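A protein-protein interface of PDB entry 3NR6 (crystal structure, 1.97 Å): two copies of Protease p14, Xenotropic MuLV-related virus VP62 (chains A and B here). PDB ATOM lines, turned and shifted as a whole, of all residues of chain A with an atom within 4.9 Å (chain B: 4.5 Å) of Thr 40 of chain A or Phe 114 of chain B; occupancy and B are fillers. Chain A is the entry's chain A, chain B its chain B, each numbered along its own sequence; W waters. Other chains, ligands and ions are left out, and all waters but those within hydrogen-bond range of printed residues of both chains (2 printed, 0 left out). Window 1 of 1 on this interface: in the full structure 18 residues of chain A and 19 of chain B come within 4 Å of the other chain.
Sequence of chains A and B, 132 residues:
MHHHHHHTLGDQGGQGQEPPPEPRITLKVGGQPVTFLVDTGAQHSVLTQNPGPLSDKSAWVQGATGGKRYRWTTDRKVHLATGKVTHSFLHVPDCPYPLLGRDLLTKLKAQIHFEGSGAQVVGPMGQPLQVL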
ATOM      1  N   VAL A  38       5.374  10.503 -14.326  1.00  0.00           N
ATOM      2  CA  VAL A  38       6.801  10.198 -14.297  1.00  0.00           C
ATOM      3  C   VAL A  38       7.481  11.554 -14.360  1.00  0.00           C
ATOM      4  O   VAL A  38       7.347  12.262 -15.352  1.00  0.00           O
ATOM      5  CB  VAL A  38       7.213   9.235 -15.442  1.00  0.00           C
ATOM      6  CG1 VAL A  38       8.638   8.733 -15.228  1.00  0.00           C
ATOM      7  CG2 VAL A  38       6.236   8.071 -15.487  1.00  0.00           C
ATOM      8  N   ASP A  39       8.147  11.930 -13.242  1.00  0.00           N
ATOM      9  CA  ASP A  39       8.581  13.308 -12.987  1.00  0.00           C
ATOM     10  C   ASP A  39      10.086  13.341 -12.722  1.00  0.00           C
ATOM     11  O   ASP A  39      10.543  13.082 -11.588  1.00  0.00           O
ATOM     12  CB  ASP A  39       7.839  13.883 -11.771  1.00  0.00           C
ATOM     13  CG  ASP A  39       8.110  15.372 -11.565  1.00  0.00           C
ATOM     14  OD1 ASP A  39       8.929  16.011 -12.304  1.00  0.00           O
ATOM     15  OD2 ASP A  39       7.460  15.934 -10.636  1.00  0.00           O
ATOM     16  N   THR A  40      10.838  13.685 -13.758  1.00  0.00           N
ATOM     17  CA  THR A  40      12.313  13.703 -13.687  1.00  0.00           C
ATOM     18  C   THR A  40      12.745  14.866 -12.789  1.00  0.00           C
ATOM     19  O   THR A  40      13.894  14.939 -12.336  1.00  0.00           O
ATOM     20  CB  THR A  40      12.922  13.883 -15.074  1.00  0.00           C
ATOM     21  OG1 THR A  40      12.358  15.062 -15.643  1.00  0.00           O
ATOM     22  CG2 THR A  40      12.555  12.682 -15.942  1.00  0.00           C
ATOM     23  N   GLY A  41      11.821  15.806 -12.552  1.00  0.00           N
ATOM     24  CA  GLY A  41      12.051  16.891 -11.607  1.00  0.00           C
ATOM     25  C   GLY A  41      11.932  16.509 -10.120  1.00  0.00           C
ATOM     26  O   GLY A  41      12.193  17.337  -9.265  1.00  0.00           O
ATOM     27  N   ALA A  42      11.516  15.282  -9.807  1.00  0.00           N
ATOM     28  CA  ALA A  42      11.348  14.872  -8.417  1.00  0.00           C
ATOM     29  C   ALA A  42      12.502  13.916  -8.021  1.00  0.00           C
ATOM     30  O   ALA A  42      12.729  12.914  -8.707  1.00  0.00           O
ATOM     31  CB  ALA A  42       9.949  14.239  -8.205  1.00  0.00           C
ATOM     32  N   ARG A 102      13.161  10.350  -9.621  1.00  0.00           N
ATOM     33  CA  ARG A 102      14.433   9.856 -10.071  1.00  0.00           C
ATOM     34  C   ARG A 102      14.915   8.655  -9.292  1.00  0.00           C
ATOM     35  O   ARG A 102      15.629   7.844  -9.882  1.00  0.00           O
ATOM     36  CB  ARG A 102      15.504  10.949 -10.000  1.00  0.00           C
ATOM     37  CG  ARG A 102      15.140  12.159 -10.856  1.00  0.00           C
ATOM     38  CD  ARG A 102      16.368  13.039 -11.035  1.00  0.00           C
ATOM     39  NE  ARG A 102      16.724  13.722  -9.815  1.00  0.00           N
ATOM     40  CZ  ARG A 102      16.229  14.887  -9.383  1.00  0.00           C
ATOM     41  NH1 ARG A 102      15.320  15.567 -10.063  1.00  0.00           N
ATOM     42  NH2 ARG A 102      16.709  15.424  -8.271  1.00  0.00           N
ATOM     43  N   LEU A 105      13.178   5.842 -11.150  1.00  0.00           N
ATOM     44  CA  LEU A 105      13.660   5.800 -12.508  1.00  0.00           C
ATOM     45  C   LEU A 105      15.076   5.190 -12.599  1.00  0.00           C
ATOM     46  O   LEU A 105      15.389   4.469 -13.535  1.00  0.00           O
ATOM     47  CB  LEU A 105      13.624   7.223 -13.166  1.00  0.00           C
ATOM     48  CG  LEU A 105      12.173   7.759 -13.333  1.00  0.00           C
ATOM     49  CD1 LEU A 105      12.108   9.302 -13.584  1.00  0.00           C
ATOM     50  CD2 LEU A 105      11.530   7.059 -14.523  1.00  0.00           C
ATOM     51  N   THR A 106      15.956   5.538 -11.669  1.00  0.00           N
ATOM     52  CA  THR A 106      17.305   5.078 -11.741  1.00  0.00           C
ATOM     53  C   THR A 106      17.345   3.591 -11.353  1.00  0.00           C
ATOM     54  O   THR A 106      18.071   2.807 -11.948  1.00  0.00           O
ATOM     55  CB  THR A 106      18.331   5.970 -10.890  1.00  0.00           C
ATOM     56  OG1 THR A 106      17.857   6.122  -9.563  1.00  0.00           O
ATOM     57  CG2 THR A 106      18.487   7.395 -11.501  1.00  0.00           C
ATOM     58  N   LYS A 109      16.037   1.806 -14.353  1.00  0.00           N
ATOM     59  CA  LYS A 109      16.779   2.125 -15.604  1.00  0.00           C
ATOM     60  C   LYS A 109      15.743   2.401 -16.693  1.00  0.00           C
ATOM     61  O   LYS A 109      15.850   1.965 -17.852  1.00  0.00           O
ATOM     62  CB  LYS A 109      17.727   0.989 -16.032  1.00  0.00           C
ATOM     63  CG  LYS A 109      18.579   0.414 -14.929  1.00  0.00           C
ATOM     64  CD  LYS A 109      19.808   1.248 -14.641  1.00  0.00           C
ATOM     65  CE  LYS A 109      20.642   0.624 -13.481  1.00  0.00           C
ATOM     66  NZ  LYS A 109      20.033   0.899 -12.116  1.00  0.00           N
ATOM     67  N   ALA A 110      14.724   3.128 -16.296  1.00  0.00           N
ATOM     68  CA  ALA A 110      13.579   3.397 -17.157  1.00  0.00           C
ATOM     69  C   ALA A 110      13.981   4.383 -18.225  1.00  0.00           C
ATOM     70  O   ALA A 110      14.976   5.120 -18.068  1.00  0.00           O
ATOM     71  CB  ALA A 110      12.390   3.955 -16.311  1.00  0.00           C
ATOM     72  N   GLN A 111      13.257   4.329 -19.344  1.00  0.00           N
ATOM     73  CA  GLN A 111      13.426   5.274 -20.425  1.00  0.00           C
ATOM     74  C   GLN A 111      12.093   5.937 -20.682  1.00  0.00           C
ATOM     75  O   GLN A 111      11.022   5.297 -20.594  1.00  0.00           O
ATOM     76  CB  GLN A 111      13.884   4.591 -21.667  1.00  0.00           C
ATOM     77  CG  GLN A 111      15.080   3.737 -21.429  1.00  0.00           C
ATOM     78  CD  GLN A 111      15.535   3.113 -22.645  1.00  0.00           C
ATOM     79  OE1 GLN A 111      14.855   3.182 -23.712  1.00  0.00           O
ATOM     80  NE2 GLN A 111      16.713   2.489 -22.557  1.00  0.00           N
ATOM     81  N   ILE A 112      12.138   7.226 -20.978  1.00  0.00           N
ATOM     82  CA  ILE A 112      10.918   7.965 -21.295  1.00  0.00           C
ATOM     83  C   ILE A 112      11.019   8.417 -22.705  1.00  0.00           C
ATOM     84  O   ILE A 112      11.977   9.100 -23.087  1.00  0.00           O
ATOM     85  CB  ILE A 112      10.694   9.215 -20.338  1.00  0.00           C
ATOM     86  CG1 ILE A 112      10.771   8.802 -18.887  1.00  0.00           C
ATOM     87  CG2 ILE A 112       9.356   9.926 -20.669  1.00  0.00           C
ATOM     88  CD1 ILE A 112      10.941   9.983 -17.841  1.00  0.00           C
ATOM     89  N   PRO B  23      18.432  14.794 -14.651  1.00  0.00           N
ATOM     90  CA  PRO B  23      18.981  14.961 -16.008  1.00  0.00           C
ATOM     91  C   PRO B  23      19.145  16.426 -16.322  1.00  0.00           C
ATOM     92  O   PRO B  23      18.164  17.193 -16.231  1.00  0.00           O
ATOM     93  CB  PRO B  23      17.922  14.318 -16.923  1.00  0.00           C
ATOM     94  CG  PRO B  23      16.637  14.227 -16.086  1.00  0.00           C
ATOM     95  CD  PRO B  23      16.991  14.444 -14.656  1.00  0.00           C
ATOM     96  N   LEU B  37      17.345  21.841 -16.141  1.00  0.00           N
ATOM     97  CA  LEU B  37      16.812  20.566 -15.695  1.00  0.00           C
ATOM     98  C   LEU B  37      15.859  20.054 -16.807  1.00  0.00           C
ATOM     99  O   LEU B  37      15.004  20.791 -17.290  1.00  0.00           O
ATOM    100  CB  LEU B  37      16.021  20.727 -14.381  1.00  0.00           C
ATOM    101  CG  LEU B  37      15.225  19.445 -13.958  1.00  0.00           C
ATOM    102  CD1 LEU B  37      16.265  18.312 -13.641  1.00  0.00           C
ATOM    103  CD2 LEU B  37      14.442  19.757 -12.656  1.00  0.00           C
ATOM    104  N   VAL B  38      15.962  18.792 -17.184  1.00  0.00           N
ATOM    105  CA  VAL B  38      14.975  18.244 -18.134  1.00  0.00           C
ATOM    106  C   VAL B  38      13.875  17.696 -17.217  1.00  0.00           C
ATOM    107  O   VAL B  38      14.119  16.729 -16.456  1.00  0.00           O
ATOM    108  CB  VAL B  38      15.592  17.154 -19.010  1.00  0.00           C
ATOM    109  CG1 VAL B  38      14.536  16.514 -19.892  1.00  0.00           C
ATOM    110  CG2 VAL B  38      16.717  17.726 -19.839  1.00  0.00           C
ATOM    111  N   ASP B  39      12.698  18.341 -17.256  1.00  0.00           N
ATOM    112  CA  ASP B  39      11.658  18.223 -16.203  1.00  0.00           C
ATOM    113  C   ASP B  39      10.349  17.790 -16.857  1.00  0.00           C
ATOM    114  O   ASP B  39       9.613  18.632 -17.452  1.00  0.00           O
ATOM    115  CB  ASP B  39      11.445  19.580 -15.515  1.00  0.00           C
ATOM    116  CG  ASP B  39      10.556  19.486 -14.212  1.00  0.00           C
ATOM    117  OD1 ASP B  39       9.922  18.433 -13.912  1.00  0.00           O
ATOM    118  OD2 ASP B  39      10.522  20.495 -13.467  1.00  0.00           O
ATOM    119  N   THR B  40      10.070  16.497 -16.760  1.00  0.00           N
ATOM    120  CA  THR B  40       8.864  15.953 -17.407  1.00  0.00           C
ATOM    121  C   THR B  40       7.625  16.429 -16.621  1.00  0.00           C
ATOM    122  O   THR B  40       6.485  16.302 -17.083  1.00  0.00           O
ATOM    123  CB  THR B  40       8.899  14.452 -17.477  1.00  0.00           C
ATOM    124  OG1 THR B  40       9.136  13.905 -16.170  1.00  0.00           O
ATOM    125  CG2 THR B  40      10.039  13.960 -18.443  1.00  0.00           C
ATOM    126  N   ILE B 112      14.526  10.122 -22.646  1.00  0.00           N
ATOM    127  CA  ILE B 112      15.395  10.270 -21.483  1.00  0.00           C
ATOM    128  C   ILE B 112      15.711   8.875 -20.962  1.00  0.00           C
ATOM    129  O   ILE B 112      14.810   8.081 -20.617  1.00  0.00           O
ATOM    130  CB  ILE B 112      14.741  11.153 -20.380  1.00  0.00           C
ATOM    131  CG1 ILE B 112      14.219  12.459 -21.006  1.00  0.00           C
ATOM    132  CG2 ILE B 112      15.772  11.375 -19.225  1.00  0.00           C
ATOM    133  CD1 ILE B 112      13.133  13.236 -20.223  1.00  0.00           C
ATOM    134  N   HIS B 113      16.970   8.531 -20.944  1.00  0.00           N
ATOM    135  CA  HIS B 113      17.305   7.167 -20.559  1.00  0.00           C
ATOM    136  C   HIS B 113      18.029   7.259 -19.215  1.00  0.00           C
ATOM    137  O   HIS B 113      19.070   7.954 -19.110  1.00  0.00           O
ATOM    138  CB  HIS B 113      18.264   6.549 -21.588  1.00  0.00           C
ATOM    139  CG  HIS B 113      17.674   6.360 -22.954  1.00  0.00           C
ATOM    140  ND1 HIS B 113      18.183   5.458 -23.857  1.00  0.00           N
ATOM    141  CD2 HIS B 113      16.643   6.966 -23.577  1.00  0.00           C
ATOM    142  CE1 HIS B 113      17.486   5.508 -24.976  1.00  0.00           C
ATOM    143  NE2 HIS B 113      16.525   6.393 -24.821  1.00  0.00           N
ATOM    144  N   PHE B 114      17.537   6.530 -18.220  1.00  0.00           N
ATOM    145  CA  PHE B 114      18.224   6.478 -16.904  1.00  0.00           C
ATOM    146  C   PHE B 114      19.181   5.352 -16.780  1.00  0.00           C
ATOM    147  O   PHE B 114      18.818   4.213 -17.012  1.00  0.00           O
ATOM    148  CB  PHE B 114      17.183   6.398 -15.763  1.00  0.00           C
ATOM    149  CG  PHE B 114      16.524   7.695 -15.533  1.00  0.00           C
ATOM    150  CD1 PHE B 114      17.089   8.633 -14.652  1.00  0.00           C
ATOM    151  CD2 PHE B 114      15.455   8.078 -16.307  1.00  0.00           C
ATOM    152  CE1 PHE B 114      16.522   9.901 -14.520  1.00  0.00           C
ATOM    153  CE2 PHE B 114      14.856   9.331 -16.150  1.00  0.00           C
ATOM    154  CZ  PHE B 114      15.413  10.260 -15.284  1.00  0.00           C
ATOM    155  N   GLU B 115      20.397   5.640 -16.326  1.00  0.00           N
ATOM    156  CA  GLU B 115      21.193   4.553 -15.764  1.00  0.00           C
ATOM    157  C   GLU B 115      21.135   4.641 -14.232  1.00  0.00           C
ATOM    158  O   GLU B 115      20.355   5.440 -13.689  1.00  0.00           O
ATOM    159  CB  GLU B 115      22.609   4.495 -16.322  1.00  0.00           C
ATOM    160  CG  GLU B 115      23.176   2.999 -16.465  1.00  0.00           C
ATOM    161  CD  GLU B 115      22.408   2.132 -17.514  1.00  0.00           C
ATOM    162  OE1 GLU B 115      21.648   2.752 -18.309  1.00  0.00           O
ATOM    163  OE2 GLU B 115      22.542   0.865 -17.542  1.00  0.00           O
ATOM    164  N   GLY B 118      22.464   8.355 -12.878  1.00  0.00           N
ATOM    165  CA  GLY B 118      22.301   9.477 -13.798  1.00  0.00           C
ATOM    166  C   GLY B 118      21.434   9.144 -14.995  1.00  0.00           C
ATOM    167  O   GLY B 118      20.649   8.202 -14.934  1.00  0.00           O
ATOM    168  N   ALA B 119      21.584   9.908 -16.083  1.00  0.00           N
ATOM    169  CA  ALA B 119      20.650   9.863 -17.200  1.00  0.00           C
ATOM    170  C   ALA B 119      21.279  10.481 -18.463  1.00  0.00           C
ATOM    171  O   ALA B 119      22.295  11.172 -18.382  1.00  0.00           O
ATOM    172  CB  ALA B 119      19.380  10.622 -16.827  1.00  0.00           C
HETATM  173  O   HOH W   1      17.722   2.653 -19.590  1.00  0.00           O
HETATM  174  O   HOH W   2       8.556  18.645 -11.691  1.00  0.00           O
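Among the printed residues, merely in contact across the chains: Asp 39 of chain A with Thr 40 of chain B (3.3 Å), Thr 40 of chain A with Pro 23 of chain B (3.9 Å), Thr 40 of chain A with Asp 39 of chain B (3.3 Å), Thr 40 of chain A with Phe 114 of chain B (3.8 Å), Gly 41 of chain A with Leu 37 of chain B (3.9 Å), Gly 41 of chain A with Asp 39 of chain B (3.5 Å), Arg 102 of chain A with Pro 23 of chain B (3.9 Å), Leu 105 of chain A with Phe 114 of chain B (3.5 Å), Thr 106 of chain A with Phe 114 of chain B (3.7 Å), Thr 106 of chain A with Glu 115 of chain B (3.5 Å), Lys 109 of chain A with Phe 114 of chain B (3.2 Å), Lys 109 of chain A with Glu 115 of chain B (3.7 Å), Ala 110 of chain A with Ile 112 of chain B (3.9 Å), Ala 110 of chain A with His 113 of chain B (3.9 Å), Gln 111 of chain A with Ile 112 of chain B (3.1 Å) and Gln 111 of chain A with His 113 of chain B (3.6 Å).
The side-chain hydroxyl of Thr 40 of chain B lies within hydrogen-bond range of the backbone carbonyl oxygen of Val 38 of chain A (2.6 Å). OG1 of Thr 40 of chain A sits at hydrogen-bond distance from O of Val 38 of chain B. N of Thr 40 of chain B sits at hydrogen-bond distance from OG1 of Thr 40 of chain A (2.9 Å). The backbone carbonyl oxygen (O) of Ala 110 of chain A is in hydrogen-bond range of the backbone NH (N) of Phe 114 of chain B (2.9 Å). The backbone carbonyl oxygen of Ile 112 of chain A lies within hydrogen-bond range of the backbone NH of Ile 112 of chain B. The side-chain carboxylate (OD1) of Asp 39 of chain A lies close to the side-chain carboxylate (OD1) of Asp 39 of chain B, at 3.1 Å.
Thr 40 of chain A touches just these residues of chain B: Pro 23, Val 38, Asp 39, Thr 40 and Phe 114. Of the printed residues of chain B, Leu 105 of chain A touches Phe 114. Of the printed residues of chain B, Lys 109 of chain A touches Phe 114 and Glu 115. Of the printed residues of chain B, Ile 112 of chain A touches Ile 112 (2.8 Å). Of the printed residues of chain A, Pro 23 of chain B touches Thr 40 (3.9 Å) and Arg 102 (3.9 Å). Phe 114 of chain B touches just these residues of chain A: Thr 40, Leu 105, Thr 106, Lys 109 and Ala 110. Of the printed residues of chain A, Glu 115 of chain B touches Thr 106 and Lys 109. The nearest residue of chain B that does not touch Thr 40 of chain A is Leu 37 of chain B (4.3 Å). The nearest printed residue of chain A that does not touch His 113 of chain B is Ile 112 of chain A (5.0 Å).
Asp 39 of chain B touches its own counterpart, Asp 39 of chain A. Asp 39 of chain A touches Thr 40 of chain B, and with the chains exchanged Thr 40 of chain A touches Asp 39 of chain B. Thr 40 of chain B touches its own counterpart, Thr 40 of chain A. Ile 112 of chain A touches its own counterpart, Ile 112 of chain B. Positions printed for both chains: 38, 39, 40 and 112. Of the 22 pairs that touch across the chains among the printed residues, 7 have their exchanged pair printed and touching as well.
Water W2 lies within hydrogen-bond range of OD1 of Asp 39 of chain B and OD1 of Asp 39 of chain A. Water W1 lies within hydrogen-bond range of O of Lys 109 of chain A (2.6 Å), NE2 of Gln 111 of chain A (3.1 Å) and O of Phe 114 of chain B (3.2 Å).
The side-chain carboxylate (OD1) of Asp 39 of chain A sits at hydrogen-bond distance from the backbone NH (N) of Gly 41 of chain A, at 2.9 Å. The backbone carbonyl oxygen (O) of Thr 40 of chain A is in hydrogen-bond range of the guanidinium group (NH1) of Arg 102 of chain A (2.8 Å). The backbone NH (N) of Arg 102 of chain A lies within hydrogen-bond range of the backbone carbonyl oxygen (O) of Ala 42 of chain A (2.8 Å). The side-chain hydroxyl (OG1) of Thr 106 of chain A sits at hydrogen-bond distance from the backbone carbonyl oxygen (O) of Arg 102 of chain A. The backbone carbonyl oxygen (O) of Thr 106 of chain A sits at hydrogen-bond distance from the side-chain amino group (NZ) of Lys 109 of chain A (2.7 Å). O of Pro 23 of chain B sits at hydrogen-bond distance from N of Val 38 of chain B (2.9 Å).
Hydrophobic or aromatic side chains of chain B that line the printed part of chain A: Pro 23, Leu 37, His 113 and Phe 114. Among the printed residues, no Asp or Glu carboxylate lies within 4 Å of a Lys or Arg side-chain nitrogen of the other chain.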
